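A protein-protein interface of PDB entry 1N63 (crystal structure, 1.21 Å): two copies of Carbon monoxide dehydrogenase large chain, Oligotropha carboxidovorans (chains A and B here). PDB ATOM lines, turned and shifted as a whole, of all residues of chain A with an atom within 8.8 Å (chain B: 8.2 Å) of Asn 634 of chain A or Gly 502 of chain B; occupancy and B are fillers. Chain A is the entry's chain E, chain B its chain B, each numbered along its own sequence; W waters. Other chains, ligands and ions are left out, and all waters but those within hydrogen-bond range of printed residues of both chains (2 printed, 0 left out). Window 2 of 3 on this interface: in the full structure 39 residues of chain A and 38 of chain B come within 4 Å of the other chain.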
ATOM      1  N   PRO A 515     -21.074  -6.920 -16.098  1.00  0.00           N
ATOM      2  CA  PRO A 515     -20.679  -8.267 -15.648  1.00  0.00           C
ATOM      3  C   PRO A 515     -20.586  -9.277 -16.761  1.00  0.00           C
ATOM      4  O   PRO A 515     -19.719 -10.149 -16.718  1.00  0.00           O
ATOM      5  CB  PRO A 515     -21.770  -8.641 -14.647  1.00  0.00           C
ATOM      6  CG  PRO A 515     -22.250  -7.284 -14.064  1.00  0.00           C
ATOM      7  CD  PRO A 515     -22.180  -6.402 -15.269  1.00  0.00           C
ATOM      8  N   ILE A 594      -6.409  -8.981 -12.023  1.00  0.00           N
ATOM      9  CA  ILE A 594      -7.419 -10.004 -11.760  1.00  0.00           C
ATOM     10  C   ILE A 594      -6.929 -11.352 -12.313  1.00  0.00           C
ATOM     11  O   ILE A 594      -7.034 -12.369 -11.638  1.00  0.00           O
ATOM     12  CB  ILE A 594      -8.812  -9.655 -12.353  1.00  0.00           C
ATOM     13  CG1 ILE A 594      -9.345  -8.384 -11.672  1.00  0.00           C
ATOM     14  CG2 ILE A 594      -9.832 -10.811 -12.157  1.00  0.00           C
ATOM     15  CD1 ILE A 594     -10.527  -7.742 -12.405  1.00  0.00           C
ATOM     16  N   MET A 598      -6.373 -14.914 -10.334  1.00  0.00           N
ATOM     17  CA  MET A 598      -7.089 -16.141 -10.755  1.00  0.00           C
ATOM     18  C   MET A 598      -6.111 -17.276 -11.094  1.00  0.00           C
ATOM     19  O   MET A 598      -6.375 -18.454 -10.827  1.00  0.00           O
ATOM     20  CB  MET A 598      -8.040 -15.925 -11.970  1.00  0.00           C
ATOM     21  CG  MET A 598      -9.186 -14.951 -11.669  1.00  0.00           C
ATOM     22  SD  MET A 598     -10.257 -14.718 -13.065  1.00  0.00           S
ATOM     23  CE  MET A 598     -11.425 -16.057 -12.842  1.00  0.00           C
ATOM     24  N   GLU A 627     -14.108 -13.396 -19.303  1.00  0.00           N
ATOM     25  CA  GLU A 627     -13.932 -14.070 -18.027  1.00  0.00           C
ATOM     26  C   GLU A 627     -13.482 -13.115 -16.903  1.00  0.00           C
ATOM     27  O   GLU A 627     -13.947 -13.212 -15.767  1.00  0.00           O
ATOM     28  CB  GLU A 627     -12.892 -15.201 -18.178  1.00  0.00           C
ATOM     29  CG  GLU A 627     -13.395 -16.382 -18.965  1.00  0.00           C
ATOM     30  CD  GLU A 627     -12.302 -17.445 -19.227  1.00  0.00           C
ATOM     31  OE2 GLU A 627     -11.078 -17.142 -19.330  1.00  0.00           O
ATOM     32  N   LEU A 628     -12.589 -12.186 -17.220  1.00  0.00           N
ATOM     33  CA  LEU A 628     -12.059 -11.282 -16.225  1.00  0.00           C
ATOM     34  C   LEU A 628     -13.098 -10.236 -15.796  1.00  0.00           C
ATOM     35  O   LEU A 628     -13.224  -9.892 -14.611  1.00  0.00           O
ATOM     36  CB  LEU A 628     -10.777 -10.604 -16.742  1.00  0.00           C
ATOM     37  CG  LEU A 628      -9.608 -11.583 -16.984  1.00  0.00           C
ATOM     38  CD1 LEU A 628      -8.515 -10.934 -17.779  1.00  0.00           C
ATOM     39  CD2 LEU A 628      -9.130 -12.064 -15.637  1.00  0.00           C
ATOM     40  N   ALA A 629     -13.881  -9.757 -16.749  1.00  0.00           N
ATOM     41  CA  ALA A 629     -15.030  -8.889 -16.433  1.00  0.00           C
ATOM     42  C   ALA A 629     -15.999  -9.572 -15.484  1.00  0.00           C
ATOM     43  O   ALA A 629     -16.418  -9.010 -14.464  1.00  0.00           O
ATOM     44  CB  ALA A 629     -15.731  -8.554 -17.703  1.00  0.00           C
ATOM     45  N   TRP A 630     -16.339 -10.818 -15.720  1.00  0.00           N
ATOM     46  CA  TRP A 630     -17.230 -11.528 -14.815  1.00  0.00           C
ATOM     47  C   TRP A 630     -16.592 -11.714 -13.463  1.00  0.00           C
ATOM     48  O   TRP A 630     -17.219 -11.463 -12.462  1.00  0.00           O
ATOM     49  CB  TRP A 630     -17.625 -12.902 -15.403  1.00  0.00           C
ATOM     50  CG  TRP A 630     -18.473 -13.759 -14.522  1.00  0.00           C
ATOM     51  CD1 TRP A 630     -18.111 -14.927 -13.945  1.00  0.00           C
ATOM     52  CD2 TRP A 630     -19.726 -13.403 -13.899  1.00  0.00           C
ATOM     53  NE1 TRP A 630     -19.106 -15.396 -13.132  1.00  0.00           N
ATOM     54  CE2 TRP A 630     -20.114 -14.482 -13.098  1.00  0.00           C
ATOM     55  CE3 TRP A 630     -20.581 -12.304 -13.980  1.00  0.00           C
ATOM     56  CZ2 TRP A 630     -21.314 -14.501 -12.407  1.00  0.00           C
ATOM     57  CZ3 TRP A 630     -21.811 -12.364 -13.387  1.00  0.00           C
ATOM     58  CH2 TRP A 630     -22.156 -13.438 -12.577  1.00  0.00           C
ATOM     59  N   ALA A 631     -15.309 -12.048 -13.429  1.00  0.00           N
ATOM     60  CA  ALA A 631     -14.643 -12.280 -12.189  1.00  0.00           C
ATOM     61  C   ALA A 631     -14.583 -10.996 -11.334  1.00  0.00           C
ATOM     62  O   ALA A 631     -14.632 -11.034 -10.098  1.00  0.00           O
ATOM     63  CB  ALA A 631     -13.224 -12.802 -12.433  1.00  0.00           C
ATOM     64  N   SER A 632     -14.511  -9.838 -11.967  1.00  0.00           N
ATOM     65  CA  SER A 632     -14.470  -8.594 -11.242  1.00  0.00           C
ATOM     66  C   SER A 632     -15.718  -8.364 -10.445  1.00  0.00           C
ATOM     67  O   SER A 632     -15.677  -7.602  -9.454  1.00  0.00           O
ATOM     68  CB  SER A 632     -14.192  -7.427 -12.194  1.00  0.00           C
ATOM     69  OG  SER A 632     -15.352  -6.956 -12.826  1.00  0.00           O
ATOM     70  N   TYR A 633     -16.823  -9.000 -10.825  1.00  0.00           N
ATOM     71  CA  TYR A 633     -18.103  -8.902 -10.133  1.00  0.00           C
ATOM     72  C   TYR A 633     -18.365 -10.132  -9.267  1.00  0.00           C
ATOM     73  O   TYR A 633     -18.998  -9.990  -8.220  1.00  0.00           O
ATOM     74  CB  TYR A 633     -19.239  -8.711 -11.145  1.00  0.00           C
ATOM     75  CG  TYR A 633     -19.281  -7.372 -11.841  1.00  0.00           C
ATOM     76  CD1 TYR A 633     -18.571  -7.170 -13.002  1.00  0.00           C
ATOM     77  CD2 TYR A 633     -20.009  -6.305 -11.339  1.00  0.00           C
ATOM     78  CE1 TYR A 633     -18.647  -6.007 -13.693  1.00  0.00           C
ATOM     79  CE2 TYR A 633     -19.989  -5.053 -11.959  1.00  0.00           C
ATOM     80  CZ  TYR A 633     -19.399  -4.952 -13.203  1.00  0.00           C
ATOM     81  OH  TYR A 633     -19.575  -3.761 -13.904  1.00  0.00           O
ATOM     82  N   ASN A 634     -17.919 -11.291  -9.724  1.00  0.00           N
ATOM     83  CA  ASN A 634     -18.285 -12.602  -9.170  1.00  0.00           C
ATOM     84  C   ASN A 634     -17.267 -13.028  -8.085  1.00  0.00           C
ATOM     85  O   ASN A 634     -17.592 -13.688  -7.130  1.00  0.00           O
ATOM     86  CB  ASN A 634     -18.401 -13.626 -10.294  1.00  0.00           C
ATOM     87  CG  ASN A 634     -18.374 -15.055  -9.809  1.00  0.00           C
ATOM     88  OD1 ASN A 634     -17.335 -15.710  -9.911  1.00  0.00           O
ATOM     89  ND2 ASN A 634     -19.488 -15.541  -9.322  1.00  0.00           N
ATOM     90  N   SER A 635     -15.999 -12.768  -8.337  1.00  0.00           N
ATOM     91  CA  SER A 635     -14.934 -13.198  -7.464  1.00  0.00           C
ATOM     92  C   SER A 635     -13.867 -12.145  -7.388  1.00  0.00           C
ATOM     93  O   SER A 635     -12.751 -12.360  -7.795  1.00  0.00           O
ATOM     94  CB  SER A 635     -14.342 -14.479  -8.017  1.00  0.00           C
ATOM     95  OG  SER A 635     -15.325 -15.482  -8.145  1.00  0.00           O
ATOM     96  N   PRO A 636     -14.225 -10.957  -6.937  1.00  0.00           N
ATOM     97  CA  PRO A 636     -13.289  -9.850  -6.974  1.00  0.00           C
ATOM     98  C   PRO A 636     -12.086 -10.248  -6.097  1.00  0.00           C
ATOM     99  O   PRO A 636     -12.286 -10.611  -4.934  1.00  0.00           O
ATOM    100  CB  PRO A 636     -14.147  -8.691  -6.420  1.00  0.00           C
ATOM    101  CG  PRO A 636     -15.251  -9.375  -5.666  1.00  0.00           C
ATOM    102  CD  PRO A 636     -15.547 -10.582  -6.394  1.00  0.00           C
ATOM    103  N   PRO A 637     -10.859 -10.001  -6.545  1.00  0.00           N
ATOM    104  CA  PRO A 637      -9.700 -10.240  -5.673  1.00  0.00           C
ATOM    105  C   PRO A 637      -9.807  -9.380  -4.439  1.00  0.00           C
ATOM    106  O   PRO A 637     -10.125  -8.215  -4.517  1.00  0.00           O
ATOM    107  CB  PRO A 637      -8.504  -9.861  -6.541  1.00  0.00           C
ATOM    108  CG  PRO A 637      -8.986 -10.082  -7.963  1.00  0.00           C
ATOM    109  CD  PRO A 637     -10.451  -9.707  -7.927  1.00  0.00           C
ATOM    110  N   PRO A 642     -14.212  -4.369  -6.417  1.00  0.00           N
ATOM    111  CA  PRO A 642     -15.011  -4.985  -7.471  1.00  0.00           C
ATOM    112  C   PRO A 642     -15.225  -4.089  -8.669  1.00  0.00           C
ATOM    113  O   PRO A 642     -14.973  -2.865  -8.638  1.00  0.00           O
ATOM    114  CB  PRO A 642     -16.339  -5.300  -6.786  1.00  0.00           C
ATOM    115  CG  PRO A 642     -16.028  -5.340  -5.348  1.00  0.00           C
ATOM    116  CD  PRO A 642     -14.942  -4.334  -5.135  1.00  0.00           C
ATOM    117  N   GLY A 643     -15.662  -4.731  -9.747  1.00  0.00           N
ATOM    118  CA  GLY A 643     -16.039  -4.063 -10.978  1.00  0.00           C
ATOM    119  C   GLY A 643     -14.842  -3.814 -11.866  1.00  0.00           C
ATOM    120  O   GLY A 643     -13.700  -4.152 -11.533  1.00  0.00           O
ATOM    121  N   LEU B  98     -34.387 -15.795  -7.548  1.00  0.00           N
ATOM    122  CA  LEU B  98     -33.219 -15.526  -6.729  1.00  0.00           C
ATOM    123  C   LEU B  98     -32.827 -16.662  -5.784  1.00  0.00           C
ATOM    124  O   LEU B  98     -31.659 -16.739  -5.375  1.00  0.00           O
ATOM    125  CB  LEU B  98     -33.366 -14.229  -5.986  1.00  0.00           C
ATOM    126  CG  LEU B  98     -33.565 -12.993  -6.900  1.00  0.00           C
ATOM    127  CD1 LEU B  98     -33.924 -11.785  -6.049  1.00  0.00           C
ATOM    128  CD2 LEU B  98     -32.332 -12.746  -7.754  1.00  0.00           C
ATOM    129  N   PRO B 348     -29.308 -13.861  -0.427  1.00  0.00           N
ATOM    130  CA  PRO B 348     -28.001 -14.228  -0.993  1.00  0.00           C
ATOM    131  C   PRO B 348     -27.983 -15.720  -1.329  1.00  0.00           C
ATOM    132  O   PRO B 348     -28.637 -16.503  -0.641  1.00  0.00           O
ATOM    133  CB  PRO B 348     -27.022 -13.925   0.127  1.00  0.00           C
ATOM    134  CG  PRO B 348     -27.760 -12.981   1.048  1.00  0.00           C
ATOM    135  CD  PRO B 348     -29.172 -13.465   0.971  1.00  0.00           C
ATOM    136  N   SER B 349     -27.328 -16.110  -2.424  1.00  0.00           N
ATOM    137  CA  SER B 349     -27.505 -17.436  -3.006  1.00  0.00           C
ATOM    138  C   SER B 349     -27.021 -18.594  -2.152  1.00  0.00           C
ATOM    139  O   SER B 349     -27.573 -19.687  -2.278  1.00  0.00           O
ATOM    140  CB  SER B 349     -26.753 -17.500  -4.343  1.00  0.00           C
ATOM    141  OG  SER B 349     -25.400 -17.818  -4.146  1.00  0.00           O
ATOM    142  N   LYS B 350     -26.190 -18.341  -1.152  1.00  0.00           N
ATOM    143  CA  LYS B 350     -25.714 -19.391  -0.281  1.00  0.00           C
ATOM    144  C   LYS B 350     -26.550 -19.555   0.984  1.00  0.00           C
ATOM    145  O   LYS B 350     -26.188 -20.340   1.864  1.00  0.00           O
ATOM    146  CB  LYS B 350     -24.228 -19.157   0.044  1.00  0.00           C
ATOM    147  CG  LYS B 350     -23.298 -19.256  -1.183  1.00  0.00           C
ATOM    148  CD  LYS B 350     -21.845 -18.900  -0.860  1.00  0.00           C
ATOM    149  CE  LYS B 350     -20.959 -18.904  -2.094  1.00  0.00           C
ATOM    150  NZ  LYS B 350     -19.605 -18.393  -1.786  1.00  0.00           N
ATOM    151  N   SER B 495     -17.717 -10.413   0.105  1.00  0.00           N
ATOM    152  CA  SER B 495     -17.641 -11.222  -1.100  1.00  0.00           C
ATOM    153  C   SER B 495     -17.408 -12.697  -0.800  1.00  0.00           C
ATOM    154  O   SER B 495     -17.649 -13.538  -1.661  1.00  0.00           O
ATOM    155  CB  SER B 495     -16.566 -10.665  -2.056  1.00  0.00           C
ATOM    156  OG  SER B 495     -15.335 -10.517  -1.381  1.00  0.00           O
ATOM    157  N   LYS B 496     -16.854 -13.019   0.356  1.00  0.00           N
ATOM    158  CA  LYS B 496     -16.585 -14.408   0.669  1.00  0.00           C
ATOM    159  C   LYS B 496     -17.865 -15.233   0.508  1.00  0.00           C
ATOM    160  O   LYS B 496     -17.860 -16.343   0.020  1.00  0.00           O
ATOM    161  CB  LYS B 496     -16.035 -14.544   2.091  1.00  0.00           C
ATOM    162  CG  LYS B 496     -15.942 -15.969   2.561  1.00  0.00           C
ATOM    163  N   CYS B 498     -21.489 -13.629   0.280  1.00  0.00           N
ATOM    164  CA  CYS B 498     -22.709 -12.916  -0.072  1.00  0.00           C
ATOM    165  C   CYS B 498     -22.696 -12.571  -1.533  1.00  0.00           C
ATOM    166  O   CYS B 498     -21.837 -11.809  -1.991  1.00  0.00           O
ATOM    167  CB  CYS B 498     -22.852 -11.641   0.779  1.00  0.00           C
ATOM    168  SG  CYS B 498     -23.191 -12.033   2.525  1.00  0.00           S
ATOM    169  N   ASP B 499     -23.652 -13.135  -2.260  1.00  0.00           N
ATOM    170  CA  ASP B 499     -23.830 -12.850  -3.659  1.00  0.00           C
ATOM    171  C   ASP B 499     -25.291 -13.015  -4.044  1.00  0.00           C
ATOM    172  O   ASP B 499     -26.009 -13.795  -3.458  1.00  0.00           O
ATOM    173  CB  ASP B 499     -22.954 -13.842  -4.499  1.00  0.00           C
ATOM    174  CG  ASP B 499     -23.459 -15.264  -4.471  1.00  0.00           C
ATOM    175  OD1 ASP B 499     -23.062 -15.975  -3.532  1.00  0.00           O
ATOM    176  OD2 ASP B 499     -24.223 -15.692  -5.349  1.00  0.00           O
ATOM    177  N   ILE B 500     -25.669 -12.292  -5.094  1.00  0.00           N
ATOM    178  CA  ILE B 500     -26.987 -12.434  -5.711  1.00  0.00           C
ATOM    179  C   ILE B 500     -26.769 -13.032  -7.100  1.00  0.00           C
ATOM    180  O   ILE B 500     -26.139 -12.397  -7.938  1.00  0.00           O
ATOM    181  CB  ILE B 500     -27.744 -11.078  -5.816  1.00  0.00           C
ATOM    182  CG1 ILE B 500     -27.984 -10.494  -4.416  1.00  0.00           C
ATOM    183  CG2 ILE B 500     -29.044 -11.292  -6.605  1.00  0.00           C
ATOM    184  CD1 ILE B 500     -29.004 -11.196  -3.651  1.00  0.00           C
ATOM    185  N   LEU B 501     -27.111 -14.315  -7.227  1.00  0.00           N
ATOM    186  CA  LEU B 501     -26.936 -15.055  -8.459  1.00  0.00           C
ATOM    187  C   LEU B 501     -25.492 -14.900  -9.020  1.00  0.00           C
ATOM    188  O   LEU B 501     -25.263 -14.697 -10.218  1.00  0.00           O
ATOM    189  CB  LEU B 501     -28.029 -14.628  -9.422  1.00  0.00           C
ATOM    190  CG  LEU B 501     -29.454 -15.086  -9.009  1.00  0.00           C
ATOM    191  CD1 LEU B 501     -30.372 -14.935 -10.158  1.00  0.00           C
ATOM    192  CD2 LEU B 501     -29.505 -16.541  -8.521  1.00  0.00           C
ATOM    193  N   GLY B 502     -24.528 -14.964  -8.119  1.00  0.00           N
ATOM    194  CA  GLY B 502     -23.136 -14.940  -8.500  1.00  0.00           C
ATOM    195  C   GLY B 502     -22.500 -13.563  -8.575  1.00  0.00           C
ATOM    196  O   GLY B 502     -21.289 -13.489  -8.765  1.00  0.00           O
ATOM    197  N   VAL B 503     -23.248 -12.493  -8.351  1.00  0.00           N
ATOM    198  CA  VAL B 503     -22.638 -11.182  -8.263  1.00  0.00           C
ATOM    199  C   VAL B 503     -22.434 -10.826  -6.803  1.00  0.00           C
ATOM    200  O   VAL B 503     -23.379 -10.823  -5.995  1.00  0.00           O
ATOM    201  CB  VAL B 503     -23.478 -10.102  -8.959  1.00  0.00           C
ATOM    202  CG1 VAL B 503     -22.903  -8.730  -8.804  1.00  0.00           C
ATOM    203  CG2 VAL B 503     -23.727 -10.446 -10.415  1.00  0.00           C
ATOM    204  N   SER B 504     -21.182 -10.615  -6.439  1.00  0.00           N
ATOM    205  CA  SER B 504     -20.872 -10.322  -5.068  1.00  0.00           C
ATOM    206  C   SER B 504     -21.671  -9.112  -4.560  1.00  0.00           C
ATOM    207  O   SER B 504     -21.881  -8.152  -5.314  1.00  0.00           O
ATOM    208  CB  SER B 504     -19.366 -10.063  -4.936  1.00  0.00           C
ATOM    209  OG  SER B 504     -18.955 -10.028  -3.583  1.00  0.00           O
ATOM    210  N   MET B 505     -21.996  -9.082  -3.257  1.00  0.00           N
ATOM    211  CA  MET B 505     -22.841  -8.033  -2.714  1.00  0.00           C
ATOM    212  C   MET B 505     -22.147  -6.757  -2.222  1.00  0.00           C
ATOM    213  O   MET B 505     -22.232  -6.365  -1.053  1.00  0.00           O
ATOM    214  CB  MET B 505     -23.800  -8.630  -1.660  1.00  0.00           C
ATOM    215  CG  MET B 505     -24.752  -9.605  -2.310  1.00  0.00           C
ATOM    216  SD  MET B 505     -25.924 -10.380  -1.145  1.00  0.00           S
ATOM    217  CE  MET B 505     -27.126  -9.001  -0.922  1.00  0.00           C
ATOM    218  N   PHE B 506     -21.344  -6.200  -3.133  1.00  0.00           N
ATOM    219  CA  PHE B 506     -20.771  -4.887  -2.876  1.00  0.00           C
ATOM    220  C   PHE B 506     -21.798  -3.800  -3.187  1.00  0.00           C
ATOM    221  O   PHE B 506     -22.945  -4.068  -3.583  1.00  0.00           O
ATOM    222  CB  PHE B 506     -19.552  -4.706  -3.776  1.00  0.00           C
ATOM    223  CG  PHE B 506     -19.885  -4.773  -5.237  1.00  0.00           C
ATOM    224  CD1 PHE B 506     -20.299  -3.653  -5.946  1.00  0.00           C
ATOM    225  CD2 PHE B 506     -19.808  -5.965  -5.917  1.00  0.00           C
ATOM    226  CE1 PHE B 506     -20.764  -3.781  -7.244  1.00  0.00           C
ATOM    227  CE2 PHE B 506     -20.114  -6.056  -7.298  1.00  0.00           C
ATOM    228  CZ  PHE B 506     -20.675  -4.985  -7.911  1.00  0.00           C
ATOM    229  N   TYR B 563     -22.701   0.144 -11.051  1.00  0.00           N
ATOM    230  CA  TYR B 563     -23.386  -1.098 -10.766  1.00  0.00           C
ATOM    231  C   TYR B 563     -23.443  -1.257  -9.247  1.00  0.00           C
ATOM    232  O   TYR B 563     -22.479  -1.121  -8.550  1.00  0.00           O
ATOM    233  CB  TYR B 563     -22.629  -2.286 -11.377  1.00  0.00           C
ATOM    234  CG  TYR B 563     -23.443  -3.553 -11.476  1.00  0.00           C
ATOM    235  CD1 TYR B 563     -23.741  -4.337 -10.378  1.00  0.00           C
ATOM    236  CD2 TYR B 563     -24.005  -3.939 -12.682  1.00  0.00           C
ATOM    237  CE1 TYR B 563     -24.499  -5.480 -10.464  1.00  0.00           C
ATOM    238  CE2 TYR B 563     -24.698  -5.102 -12.788  1.00  0.00           C
ATOM    239  CZ  TYR B 563     -24.957  -5.848 -11.717  1.00  0.00           C
ATOM    240  OH  TYR B 563     -25.766  -6.977 -11.811  1.00  0.00           O
ATOM    241  N   LEU B 565     -26.035  -3.534  -6.047  1.00  0.00           N
ATOM    242  CA  LEU B 565     -26.890  -4.673  -5.786  1.00  0.00           C
ATOM    243  C   LEU B 565     -28.270  -4.251  -5.297  1.00  0.00           C
ATOM    244  O   LEU B 565     -29.128  -5.085  -5.075  1.00  0.00           O
ATOM    245  CB  LEU B 565     -26.221  -5.687  -4.875  1.00  0.00           C
ATOM    246  CG  LEU B 565     -25.232  -6.630  -5.591  1.00  0.00           C
ATOM    247  CD1 LEU B 565     -25.931  -7.577  -6.513  1.00  0.00           C
ATOM    248  CD2 LEU B 565     -24.130  -5.908  -6.377  1.00  0.00           C
HETATM  249  O   HOH W   1     -15.983 -13.936  -4.245  1.00  0.00           O
HETATM  250  O   HOH W   2     -19.878 -14.628  -5.814  1.00  0.00           O
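Water W2 bridges O of Asn 634 of chain A (2.8 Å) and O of Gly 502 of chain B (3.5 Å).
Water W1 bridges O of Ser 495 of chain B (3.1 Å) and O of Asn 634 of chain A (3.3 Å).
Pro 515 of chain A touches Tyr 563 of chain B (CG to CE2, 3.5 Å).
Trp 630 of chain A touches Gly 502 of chain B (CZ2 to O, 3.8 Å).
Val 503 of chain B touches Tyr 633 of chain A (C to O, 3.8 Å).
CD2 of Tyr 633 of chain A touches CZ of Phe 506 of chain B, 3.7 Å away.
Tyr 633 of chain A touches Tyr 563 of chain B (CE2 to CG, 3.8 Å).
Pro 642 of chain A touches Phe 506 of chain B.
Of the 16 printed residues of chain A, 5 touch a printed residue of chain B.
Hydrophobic or aromatic side chains of chain A that line the printed part of chain B: Pro 515, Trp 630, Tyr 633 and Pro 642.
Of the 17 printed residues of chain B, 5 touch a printed residue of chain A.
Printed residues of chain B that touch a printed residue of chain A: Gly 502, Val 503, Ser 504, Phe 506 and Tyr 563.
The backbone carbonyl oxygen (O) of Gly 502 of chain B is in hydrogen-bond range of the side-chain amide nitrogen (ND2) of Asn 634 of chain A (2.8 Å).
N of Ser 504 of chain B lies within hydrogen-bond range of O of Tyr 633 of chain A, at 2.9 Å.
No position is printed for both chains.
Of the 8 pairs that touch across the chains among the printed residues, none has its exchanged pair printed and touching as well.
Of the printed residues of chain B, Trp 630 of chain A touches Gly 502 (3.8 Å).
Of the printed residues of chain B, Asn 634 of chain A touches Gly 502.
Of the printed residues of chain B, Pro 642 of chain A touches Phe 506.
Asp 499 of chain B touches none of the printed residues of chain A.
Of chain A, only Trp 630 (3.8 Å) and Asn 634 (2.8 Å) come within 4 Å of Gly 502 of chain B.
Of the printed residues of chain A, Tyr 563 of chain B touches Pro 515 (3.5 Å) and Tyr 633 (3.8 Å).
The nearest printed residue of chain B that does not touch Asn 634 of chain A is Ser 504 of chain B (4.4 Å).
OD2 of Asp 499 of chain B sits at hydrogen-bond distance from N of Gly 502 of chain B.
The side-chain hydroxyl (OG) of Ser 635 of chain A sits at hydrogen-bond distance from the side-chain amide oxygen (OD1) of Asn 634 of chain A, at 2.7 Å.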
